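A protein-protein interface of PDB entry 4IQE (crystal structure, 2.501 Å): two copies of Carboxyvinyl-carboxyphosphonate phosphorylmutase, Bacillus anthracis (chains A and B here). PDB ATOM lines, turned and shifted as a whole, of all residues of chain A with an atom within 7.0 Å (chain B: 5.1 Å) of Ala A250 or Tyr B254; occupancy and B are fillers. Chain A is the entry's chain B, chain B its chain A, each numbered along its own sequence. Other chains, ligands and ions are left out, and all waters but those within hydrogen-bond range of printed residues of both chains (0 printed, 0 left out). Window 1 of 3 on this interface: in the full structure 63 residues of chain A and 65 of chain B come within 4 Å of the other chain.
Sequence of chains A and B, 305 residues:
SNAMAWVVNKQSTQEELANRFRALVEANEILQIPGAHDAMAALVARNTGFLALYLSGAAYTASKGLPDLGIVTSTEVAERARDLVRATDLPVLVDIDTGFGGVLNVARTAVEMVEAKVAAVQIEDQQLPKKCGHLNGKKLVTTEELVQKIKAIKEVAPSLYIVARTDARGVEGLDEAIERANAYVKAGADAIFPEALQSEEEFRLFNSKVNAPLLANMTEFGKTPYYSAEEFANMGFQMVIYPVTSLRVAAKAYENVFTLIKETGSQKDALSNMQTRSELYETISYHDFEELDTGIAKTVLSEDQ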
ATOM      1  N   HIS A  37      10.777   6.442 -27.289  1.00  0.00           N
ATOM      2  CA  HIS A  37      12.231   6.569 -27.320  1.00  0.00           C
ATOM      3  C   HIS A  37      12.775   6.838 -28.721  1.00  0.00           C
ATOM      4  O   HIS A  37      13.884   7.349 -28.873  1.00  0.00           O
ATOM      5  CB  HIS A  37      12.899   5.334 -26.708  1.00  0.00           C
ATOM      6  CG  HIS A  37      12.654   4.069 -27.469  1.00  0.00           C
ATOM      7  ND1 HIS A  37      13.400   3.708 -28.571  1.00  0.00           N
ATOM      8  CD2 HIS A  37      11.752   3.078 -27.286  1.00  0.00           C
ATOM      9  CE1 HIS A  37      12.966   2.550 -29.033  1.00  0.00           C
ATOM     10  NE2 HIS A  37      11.965   2.146 -28.271  1.00  0.00           N
ATOM     11  N   ASP A  38      11.993   6.497 -29.741  1.00  0.00           N
ATOM     12  CA  ASP A  38      12.382   6.783 -31.119  1.00  0.00           C
ATOM     13  C   ASP A  38      11.176   7.137 -31.985  1.00  0.00           C
ATOM     14  O   ASP A  38      10.035   7.076 -31.529  1.00  0.00           O
ATOM     15  CB  ASP A  38      13.162   5.611 -31.723  1.00  0.00           C
ATOM     16  CG  ASP A  38      12.321   4.359 -31.869  1.00  0.00           C
ATOM     17  OD1 ASP A  38      11.336   4.206 -31.119  1.00  0.00           O
ATOM     18  OD2 ASP A  38      12.647   3.520 -32.735  1.00  0.00           O
ATOM     19  N   ALA A  39      11.439   7.507 -33.234  1.00  0.00           N
ATOM     20  CA  ALA A  39      10.396   7.984 -34.138  1.00  0.00           C
ATOM     21  C   ALA A  39       9.368   6.911 -34.487  1.00  0.00           C
ATOM     22  O   ALA A  39       8.195   7.217 -34.702  1.00  0.00           O
ATOM     23  CB  ALA A  39      11.014   8.560 -35.403  1.00  0.00           C
ATOM     24  N   MET A  40       9.809   5.659 -34.546  1.00  0.00           N
ATOM     25  CA  MET A  40       8.907   4.550 -34.839  1.00  0.00           C
ATOM     26  C   MET A  40       7.857   4.393 -33.743  1.00  0.00           C
ATOM     27  O   MET A  40       6.671   4.235 -34.027  1.00  0.00           O
ATOM     28  CB  MET A  40       9.688   3.246 -35.018  1.00  0.00           C
ATOM     29  CG  MET A  40       8.814   2.001 -35.092  1.00  0.00           C
ATOM     30  SD  MET A  40       7.428   2.110 -36.461  1.00  0.00           S
ATOM     31  CE  MET A  40       8.556   2.164 -38.045  1.00  0.00           C
ATOM     32  N   ALA A  41       8.304   4.445 -32.492  1.00  0.00           N
ATOM     33  CA  ALA A  41       7.401   4.356 -31.350  1.00  0.00           C
ATOM     34  C   ALA A  41       6.462   5.556 -31.312  1.00  0.00           C
ATOM     35  O   ALA A  41       5.323   5.452 -30.861  1.00  0.00           O
ATOM     36  CB  ALA A  41       8.192   4.255 -30.055  1.00  0.00           C
ATOM     37  N   ALA A  42       6.952   6.696 -31.789  1.00  0.00           N
ATOM     38  CA  ALA A  42       6.151   7.911 -31.848  1.00  0.00           C
ATOM     39  C   ALA A  42       5.045   7.780 -32.891  1.00  0.00           C
ATOM     40  O   ALA A  42       3.932   8.262 -32.691  1.00  0.00           O
ATOM     41  CB  ALA A  42       7.034   9.109 -32.156  1.00  0.00           C
ATOM     42  N   VAL A  44       3.544   4.962 -33.948  1.00  0.00           N
ATOM     43  CA  VAL A  44       2.525   4.029 -33.485  1.00  0.00           C
ATOM     44  C   VAL A  44       1.651   4.666 -32.406  1.00  0.00           C
ATOM     45  O   VAL A  44       0.456   4.386 -32.317  1.00  0.00           O
ATOM     46  CB  VAL A  44       3.156   2.732 -32.944  1.00  0.00           C
ATOM     47  CG1 VAL A  44       2.082   1.701 -32.646  1.00  0.00           C
ATOM     48  CG2 VAL A  44       4.158   2.177 -33.945  1.00  0.00           C
ATOM     49  N   ALA A  45       2.254   5.530 -31.596  1.00  0.00           N
ATOM     50  CA  ALA A  45       1.526   6.226 -30.540  1.00  0.00           C
ATOM     51  C   ALA A  45       0.453   7.142 -31.122  1.00  0.00           C
ATOM     52  O   ALA A  45      -0.663   7.206 -30.608  1.00  0.00           O
ATOM     53  CB  ALA A  45       2.486   7.017 -29.666  1.00  0.00           C
ATOM     54  N   THR A  48      -2.263   5.110 -32.579  1.00  0.00           N
ATOM     55  CA  THR A  48      -3.068   4.556 -31.500  1.00  0.00           C
ATOM     56  C   THR A  48      -4.102   5.584 -31.052  1.00  0.00           C
ATOM     57  O   THR A  48      -5.159   5.233 -30.528  1.00  0.00           O
ATOM     58  CB  THR A  48      -2.195   4.139 -30.304  1.00  0.00           C
ATOM     59  OG1 THR A  48      -1.057   3.406 -30.772  1.00  0.00           O
ATOM     60  CG2 THR A  48      -2.986   3.269 -29.348  1.00  0.00           C
ATOM     61  N   THR A 245       8.063   2.913 -20.991  1.00  0.00           N
ATOM     62  CA  THR A 245       7.242   1.750 -21.315  1.00  0.00           C
ATOM     63  C   THR A 245       7.536   1.172 -22.701  1.00  0.00           C
ATOM     64  O   THR A 245       7.600  -0.044 -22.871  1.00  0.00           O
ATOM     65  CB  THR A 245       5.739   2.083 -21.219  1.00  0.00           C
ATOM     66  OG1 THR A 245       5.460   2.684 -19.948  1.00  0.00           O
ATOM     67  CG2 THR A 245       4.901   0.828 -21.376  1.00  0.00           C
ATOM     68  N   SER A 246       7.719   2.050 -23.684  1.00  0.00           N
ATOM     69  CA  SER A 246       7.988   1.625 -25.054  1.00  0.00           C
ATOM     70  C   SER A 246       9.327   0.906 -25.169  1.00  0.00           C
ATOM     71  O   SER A 246       9.467  -0.043 -25.938  1.00  0.00           O
ATOM     72  CB  SER A 246       7.961   2.820 -26.005  1.00  0.00           C
ATOM     73  OG  SER A 246       8.978   3.750 -25.688  1.00  0.00           O
ATOM     74  N   LEU A 247      10.312   1.368 -24.409  1.00  0.00           N
ATOM     75  CA  LEU A 247      11.631   0.751 -24.422  1.00  0.00           C
ATOM     76  C   LEU A 247      11.593  -0.632 -23.780  1.00  0.00           C
ATOM     77  O   LEU A 247      12.275  -1.553 -24.228  1.00  0.00           O
ATOM     78  CB  LEU A 247      12.633   1.637 -23.684  1.00  0.00           C
ATOM     79  CG  LEU A 247      14.042   1.067 -23.530  1.00  0.00           C
ATOM     80  CD1 LEU A 247      14.881   1.380 -24.758  1.00  0.00           C
ATOM     81  CD2 LEU A 247      14.695   1.593 -22.264  1.00  0.00           C
ATOM     82  N   ARG A 248      10.785  -0.770 -22.734  1.00  0.00           N
ATOM     83  CA  ARG A 248      10.710  -2.020 -21.984  1.00  0.00           C
ATOM     84  C   ARG A 248      10.137  -3.174 -22.805  1.00  0.00           C
ATOM     85  O   ARG A 248      10.622  -4.302 -22.721  1.00  0.00           O
ATOM     86  CB  ARG A 248       9.909  -1.833 -20.692  1.00  0.00           C
ATOM     87  CG  ARG A 248      10.591  -0.931 -19.674  1.00  0.00           C
ATOM     88  CD  ARG A 248       9.974  -1.075 -18.292  1.00  0.00           C
ATOM     89  NE  ARG A 248      10.896  -0.652 -17.241  1.00  0.00           N
ATOM     90  CZ  ARG A 248      10.623   0.275 -16.328  1.00  0.00           C
ATOM     91  NH1 ARG A 248       9.446   0.883 -16.326  1.00  0.00           N
ATOM     92  NH2 ARG A 248      11.530   0.591 -15.413  1.00  0.00           N
ATOM     93  N   VAL A 249       9.109  -2.889 -23.598  1.00  0.00           N
ATOM     94  CA  VAL A 249       8.488  -3.913 -24.433  1.00  0.00           C
ATOM     95  C   VAL A 249       9.342  -4.253 -25.652  1.00  0.00           C
ATOM     96  O   VAL A 249       9.282  -5.368 -26.169  1.00  0.00           O
ATOM     97  CB  VAL A 249       7.068  -3.508 -24.891  1.00  0.00           C
ATOM     98  CG1 VAL A 249       6.128  -3.433 -23.702  1.00  0.00           C
ATOM     99  CG2 VAL A 249       7.096  -2.187 -25.641  1.00  0.00           C
ATOM    100  N   ALA A 250      10.138  -3.289 -26.103  1.00  0.00           N
ATOM    101  CA  ALA A 250      11.002  -3.494 -27.258  1.00  0.00           C
ATOM    102  C   ALA A 250      12.155  -4.426 -26.908  1.00  0.00           C
ATOM    103  O   ALA A 250      12.535  -5.284 -27.703  1.00  0.00           O
ATOM    104  CB  ALA A 250      11.531  -2.163 -27.769  1.00  0.00           C
ATOM    105  N   ALA A 251      12.699  -4.252 -25.708  1.00  0.00           N
ATOM    106  CA  ALA A 251      13.835  -5.040 -25.245  1.00  0.00           C
ATOM    107  C   ALA A 251      13.488  -6.518 -25.110  1.00  0.00           C
ATOM    108  O   ALA A 251      14.212  -7.381 -25.610  1.00  0.00           O
ATOM    109  CB  ALA A 251      14.347  -4.493 -23.922  1.00  0.00           C
ATOM    110  N   LYS A 252      12.381  -6.804 -24.431  1.00  0.00           N
ATOM    111  CA  LYS A 252      11.930  -8.178 -24.233  1.00  0.00           C
ATOM    112  C   LYS A 252      11.592  -8.827 -25.571  1.00  0.00           C
ATOM    113  O   LYS A 252      11.724 -10.039 -25.737  1.00  0.00           O
ATOM    114  CB  LYS A 252      10.712  -8.211 -23.306  1.00  0.00           C
ATOM    115  CG  LYS A 252      10.312  -9.604 -22.839  1.00  0.00           C
ATOM    116  CD  LYS A 252      10.823  -9.895 -21.434  1.00  0.00           C
ATOM    117  CE  LYS A 252      10.309 -11.236 -20.929  1.00  0.00           C
ATOM    118  NZ  LYS A 252      10.660 -11.471 -19.501  1.00  0.00           N
ATOM    119  N   ALA A 253      11.157  -8.007 -26.523  1.00  0.00           N
ATOM    120  CA  ALA A 253      10.880  -8.481 -27.871  1.00  0.00           C
ATOM    121  C   ALA A 253      12.175  -8.895 -28.559  1.00  0.00           C
ATOM    122  O   ALA A 253      12.211  -9.890 -29.284  1.00  0.00           O
ATOM    123  CB  ALA A 253      10.166  -7.407 -28.677  1.00  0.00           C
ATOM    124  N   TYR A 254      13.235  -8.125 -28.329  1.00  0.00           N
ATOM    125  CA  TYR A 254      14.552  -8.455 -28.858  1.00  0.00           C
ATOM    126  C   TYR A 254      15.031  -9.765 -28.249  1.00  0.00           C
ATOM    127  O   TYR A 254      15.565 -10.627 -28.944  1.00  0.00           O
ATOM    128  CB  TYR A 254      15.563  -7.354 -28.529  1.00  0.00           C
ATOM    129  CG  TYR A 254      15.201  -5.977 -29.040  1.00  0.00           C
ATOM    130  CD1 TYR A 254      14.424  -5.812 -30.179  1.00  0.00           C
ATOM    131  CD2 TYR A 254      15.643  -4.838 -28.379  1.00  0.00           C
ATOM    132  CE1 TYR A 254      14.097  -4.550 -30.643  1.00  0.00           C
ATOM    133  CE2 TYR A 254      15.320  -3.575 -28.835  1.00  0.00           C
ATOM    134  CZ  TYR A 254      14.548  -3.436 -29.968  1.00  0.00           C
ATOM    135  OH  TYR A 254      14.226  -2.178 -30.423  1.00  0.00           O
ATOM    136  N   GLU A 255      14.829  -9.902 -26.943  1.00  0.00           N
ATOM    137  CA  GLU A 255      15.285 -11.067 -26.195  1.00  0.00           C
ATOM    138  C   GLU A 255      14.648 -12.356 -26.699  1.00  0.00           C
ATOM    139  O   GLU A 255      15.309 -13.389 -26.794  1.00  0.00           O
ATOM    140  CB  GLU A 255      14.991 -10.886 -24.704  1.00  0.00           C
ATOM    141  CG  GLU A 255      15.567 -11.974 -23.813  1.00  0.00           C
ATOM    142  CD  GLU A 255      15.234 -11.763 -22.349  1.00  0.00           C
ATOM    143  OE1 GLU A 255      14.225 -11.088 -22.058  1.00  0.00           O
ATOM    144  OE2 GLU A 255      15.986 -12.268 -21.488  1.00  0.00           O
ATOM    145  N   ALA B 250       9.716  -4.995 -32.586  1.00  0.00           N
ATOM    146  CA  ALA B 250       9.616  -3.808 -31.745  1.00  0.00           C
ATOM    147  C   ALA B 250       8.352  -3.009 -32.044  1.00  0.00           C
ATOM    148  O   ALA B 250       7.626  -2.616 -31.130  1.00  0.00           O
ATOM    149  CB  ALA B 250      10.851  -2.931 -31.913  1.00  0.00           C
ATOM    150  N   ALA B 251       8.094  -2.773 -33.327  1.00  0.00           N
ATOM    151  CA  ALA B 251       6.922  -2.010 -33.746  1.00  0.00           C
ATOM    152  C   ALA B 251       5.631  -2.734 -33.383  1.00  0.00           C
ATOM    153  O   ALA B 251       4.626  -2.105 -33.054  1.00  0.00           O
ATOM    154  CB  ALA B 251       6.978  -1.730 -35.239  1.00  0.00           C
ATOM    155  N   LYS B 252       5.669  -4.061 -33.445  1.00  0.00           N
ATOM    156  CA  LYS B 252       4.520  -4.881 -33.087  1.00  0.00           C
ATOM    157  C   LYS B 252       4.265  -4.803 -31.584  1.00  0.00           C
ATOM    158  O   LYS B 252       3.123  -4.893 -31.130  1.00  0.00           O
ATOM    159  CB  LYS B 252       4.753  -6.335 -33.507  1.00  0.00           C
ATOM    160  CG  LYS B 252       3.525  -7.224 -33.392  1.00  0.00           C
ATOM    161  CD  LYS B 252       2.446  -6.804 -34.377  1.00  0.00           C
ATOM    162  CE  LYS B 252       1.247  -7.739 -34.307  1.00  0.00           C
ATOM    163  NZ  LYS B 252       0.210  -7.394 -35.322  1.00  0.00           N
ATOM    164  N   ALA B 253       5.339  -4.632 -30.818  1.00  0.00           N
ATOM    165  CA  ALA B 253       5.244  -4.541 -29.366  1.00  0.00           C
ATOM    166  C   ALA B 253       4.708  -3.184 -28.922  1.00  0.00           C
ATOM    167  O   ALA B 253       3.950  -3.095 -27.956  1.00  0.00           O
ATOM    168  CB  ALA B 253       6.598  -4.810 -28.727  1.00  0.00           C
ATOM    169  N   TYR B 254       5.110  -2.132 -29.630  1.00  0.00           N
ATOM    170  CA  TYR B 254       4.609  -0.789 -29.360  1.00  0.00           C
ATOM    171  C   TYR B 254       3.106  -0.766 -29.586  1.00  0.00           C
ATOM    172  O   TYR B 254       2.355  -0.219 -28.782  1.00  0.00           O
ATOM    173  CB  TYR B 254       5.275   0.237 -30.279  1.00  0.00           C
ATOM    174  CG  TYR B 254       6.782   0.300 -30.175  1.00  0.00           C
ATOM    175  CD1 TYR B 254       7.440  -0.116 -29.025  1.00  0.00           C
ATOM    176  CD2 TYR B 254       7.546   0.779 -31.230  1.00  0.00           C
ATOM    177  CE1 TYR B 254       8.817  -0.057 -28.933  1.00  0.00           C
ATOM    178  CE2 TYR B 254       8.922   0.841 -31.145  1.00  0.00           C
ATOM    179  CZ  TYR B 254       9.552   0.421 -29.995  1.00  0.00           C
ATOM    180  OH  TYR B 254      10.924   0.481 -29.908  1.00  0.00           O
ATOM    181  N   GLU B 255       2.683  -1.374 -30.689  1.00  0.00           N
ATOM    182  CA  GLU B 255       1.274  -1.469 -31.050  1.00  0.00           C
ATOM    183  C   GLU B 255       0.440  -2.099 -29.938  1.00  0.00           C
ATOM    184  O   GLU B 255      -0.626  -1.594 -29.589  1.00  0.00           O
ATOM    185  CB  GLU B 255       1.120  -2.276 -32.341  1.00  0.00           C
ATOM    186  CG  GLU B 255      -0.313  -2.610 -32.715  1.00  0.00           C
ATOM    187  CD  GLU B 255      -0.395  -3.552 -33.900  1.00  0.00           C
ATOM    188  OE1 GLU B 255       0.668  -3.906 -34.454  1.00  0.00           O
ATOM    189  OE2 GLU B 255      -1.519  -3.942 -34.275  1.00  0.00           O
ATOM    190  N   ASN B 256       0.934  -3.201 -29.383  1.00  0.00           N
ATOM    191  CA  ASN B 256       0.234  -3.896 -28.310  1.00  0.00           C
ATOM    192  C   ASN B 256       0.079  -3.047 -27.055  1.00  0.00           C
ATOM    193  O   ASN B 256      -1.028  -2.863 -26.549  1.00  0.00           O
ATOM    194  CB  ASN B 256       0.947  -5.203 -27.961  1.00  0.00           C
ATOM    195  CG  ASN B 256       0.427  -6.379 -28.759  1.00  0.00           C
ATOM    196  OD1 ASN B 256       0.019  -6.234 -29.910  1.00  0.00           O
ATOM    197  ND2 ASN B 256       0.427  -7.556 -28.143  1.00  0.00           N
ATOM    198  N   VAL B 257       1.195  -2.526 -26.561  1.00  0.00           N
ATOM    199  CA  VAL B 257       1.198  -1.793 -25.301  1.00  0.00           C
ATOM    200  C   VAL B 257       0.514  -0.426 -25.412  1.00  0.00           C
ATOM    201  O   VAL B 257      -0.079   0.055 -24.445  1.00  0.00           O
ATOM    202  CB  VAL B 257       2.632  -1.655 -24.728  1.00  0.00           C
ATOM    203  CG1 VAL B 257       3.472  -0.706 -25.574  1.00  0.00           C
ATOM    204  CG2 VAL B 257       2.586  -1.201 -23.278  1.00  0.00           C
ATOM    205  N   PHE B 258       0.579   0.189 -26.589  1.00  0.00           N
ATOM    206  CA  PHE B 258      -0.069   1.480 -26.799  1.00  0.00           C
ATOM    207  C   PHE B 258      -1.582   1.327 -26.883  1.00  0.00           C
ATOM    208  O   PHE B 258      -2.325   2.133 -26.325  1.00  0.00           O
ATOM    209  CB  PHE B 258       0.463   2.166 -28.058  1.00  0.00           C
ATOM    210  CG  PHE B 258       1.870   2.673 -27.922  1.00  0.00           C
ATOM    211  CD1 PHE B 258       2.424   2.900 -26.673  1.00  0.00           C
ATOM    212  CD2 PHE B 258       2.638   2.928 -29.047  1.00  0.00           C
ATOM    213  CE1 PHE B 258       3.719   3.369 -26.547  1.00  0.00           C
ATOM    214  CE2 PHE B 258       3.932   3.395 -28.927  1.00  0.00           C
ATOM    215  CZ  PHE B 258       4.474   3.617 -27.676  1.00  0.00           C
ATOM    216  N   THR B 259      -2.027   0.293 -27.589  1.00  0.00           N
ATOM    217  CA  THR B 259      -3.451   0.006 -27.713  1.00  0.00           C
ATOM    218  C   THR B 259      -4.040  -0.270 -26.339  1.00  0.00           C
ATOM    219  O   THR B 259      -5.150   0.157 -26.029  1.00  0.00           O
ATOM    220  CB  THR B 259      -3.705  -1.214 -28.616  1.00  0.00           C
ATOM    221  OG1 THR B 259      -2.983  -1.063 -29.845  1.00  0.00           O
ATOM    222  CG2 THR B 259      -5.191  -1.357 -28.914  1.00  0.00           C
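A ring nitrogen (NE2) of His A37 sits at hydrogen-bond distance from the side-chain hydroxyl (OH) of Tyr B254, at 2.6 Å.
OE1 of Glu B255 is in salt-bridge range of NZ of Lys B252 (3.6 Å).
The side-chain hydroxyl of Thr B259 is in hydrogen-bond range of the backbone carbonyl oxygen of Glu B255 (2.4 Å).
A ring nitrogen (ND1) of His A37 sits close to the side-chain carboxylate of Asp A38 (3.3 Å).
The side-chain carboxylate (OD1) of Asp A38 lies close to the backbone NH (N) of Ala A41 (3.3 Å).
OD1 of Asp A38 touches OH of Tyr B254 (3.9 Å).
Ala A41 touches Phe B258.
Phe B258 touches Ala A45.
Thr B259 touches Thr A48.
Val B257 touches Thr A245 (CG2 to CG2, 3.6 Å).
O of Ser A246 touches CE1 of Tyr B254, 3.1 Å away.
Phe B258 touches Ser A246 (CZ to CB, 3.9 Å).
O of Val A249 touches CB of Ala B253 (3.7 Å).
CD1 of Tyr B254 touches CG2 of Val A249 (3.98 Å).
Ala A250 touches Tyr B254 (CB to OH, 3.5 Å).
Ala A250 touches Tyr B254, and with the chains exchanged Tyr A254 touches Ala B250.
Of the 10 printed residues of chain B, 7 touch a printed residue of chain A.
Hydrophobic or aromatic side chains of chain B that line the printed part of chain A: Ala B250, Ala B253, Tyr B254, Val B257 and Phe B258.
Hydrophobic or aromatic side chains of chain A that line the printed part of chain B: His A37, Ala A41, Val A44, Ala A45, Val A249, Ala A250 and Tyr A254.
Along chain A the printed residues that touch a printed residue of chain B span positions 37 to 254.
Among the printed residues, 17 pairs touch across the chains.
Of the printed residues of chain B, Ala A41 touches Tyr B254 (3.6 Å) and Phe B258 (3.1 Å).
Printed residues of chain B within 4 Å of Ser A246: Tyr B254 (3.1 Å) and Phe B258 (3.9 Å).
Of chain B, only Tyr B254 comes within 4 Å of Ala A250.
Of the printed residues of chain B, Tyr A254 touches Ala B250 (3.8 Å).
Ala B251 touches none of the printed residues of chain A.
Of the printed residues of chain A, Ala B253 touches Val A249 (3.7 Å).
Of the printed residues of chain A, Tyr B254 touches His A37 (2.6 Å), Asp A38 (3.9 Å), Ala A41 (3.6 Å), Ser A246 (3.1 Å), Val A249 (3.98 Å) and Ala A250 (3.5 Å).
Of the printed residues of chain A, Glu B255 touches Val A44.
The nearest printed residue of chain A that does not touch Thr B259 is Val A44 (6.4 Å).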
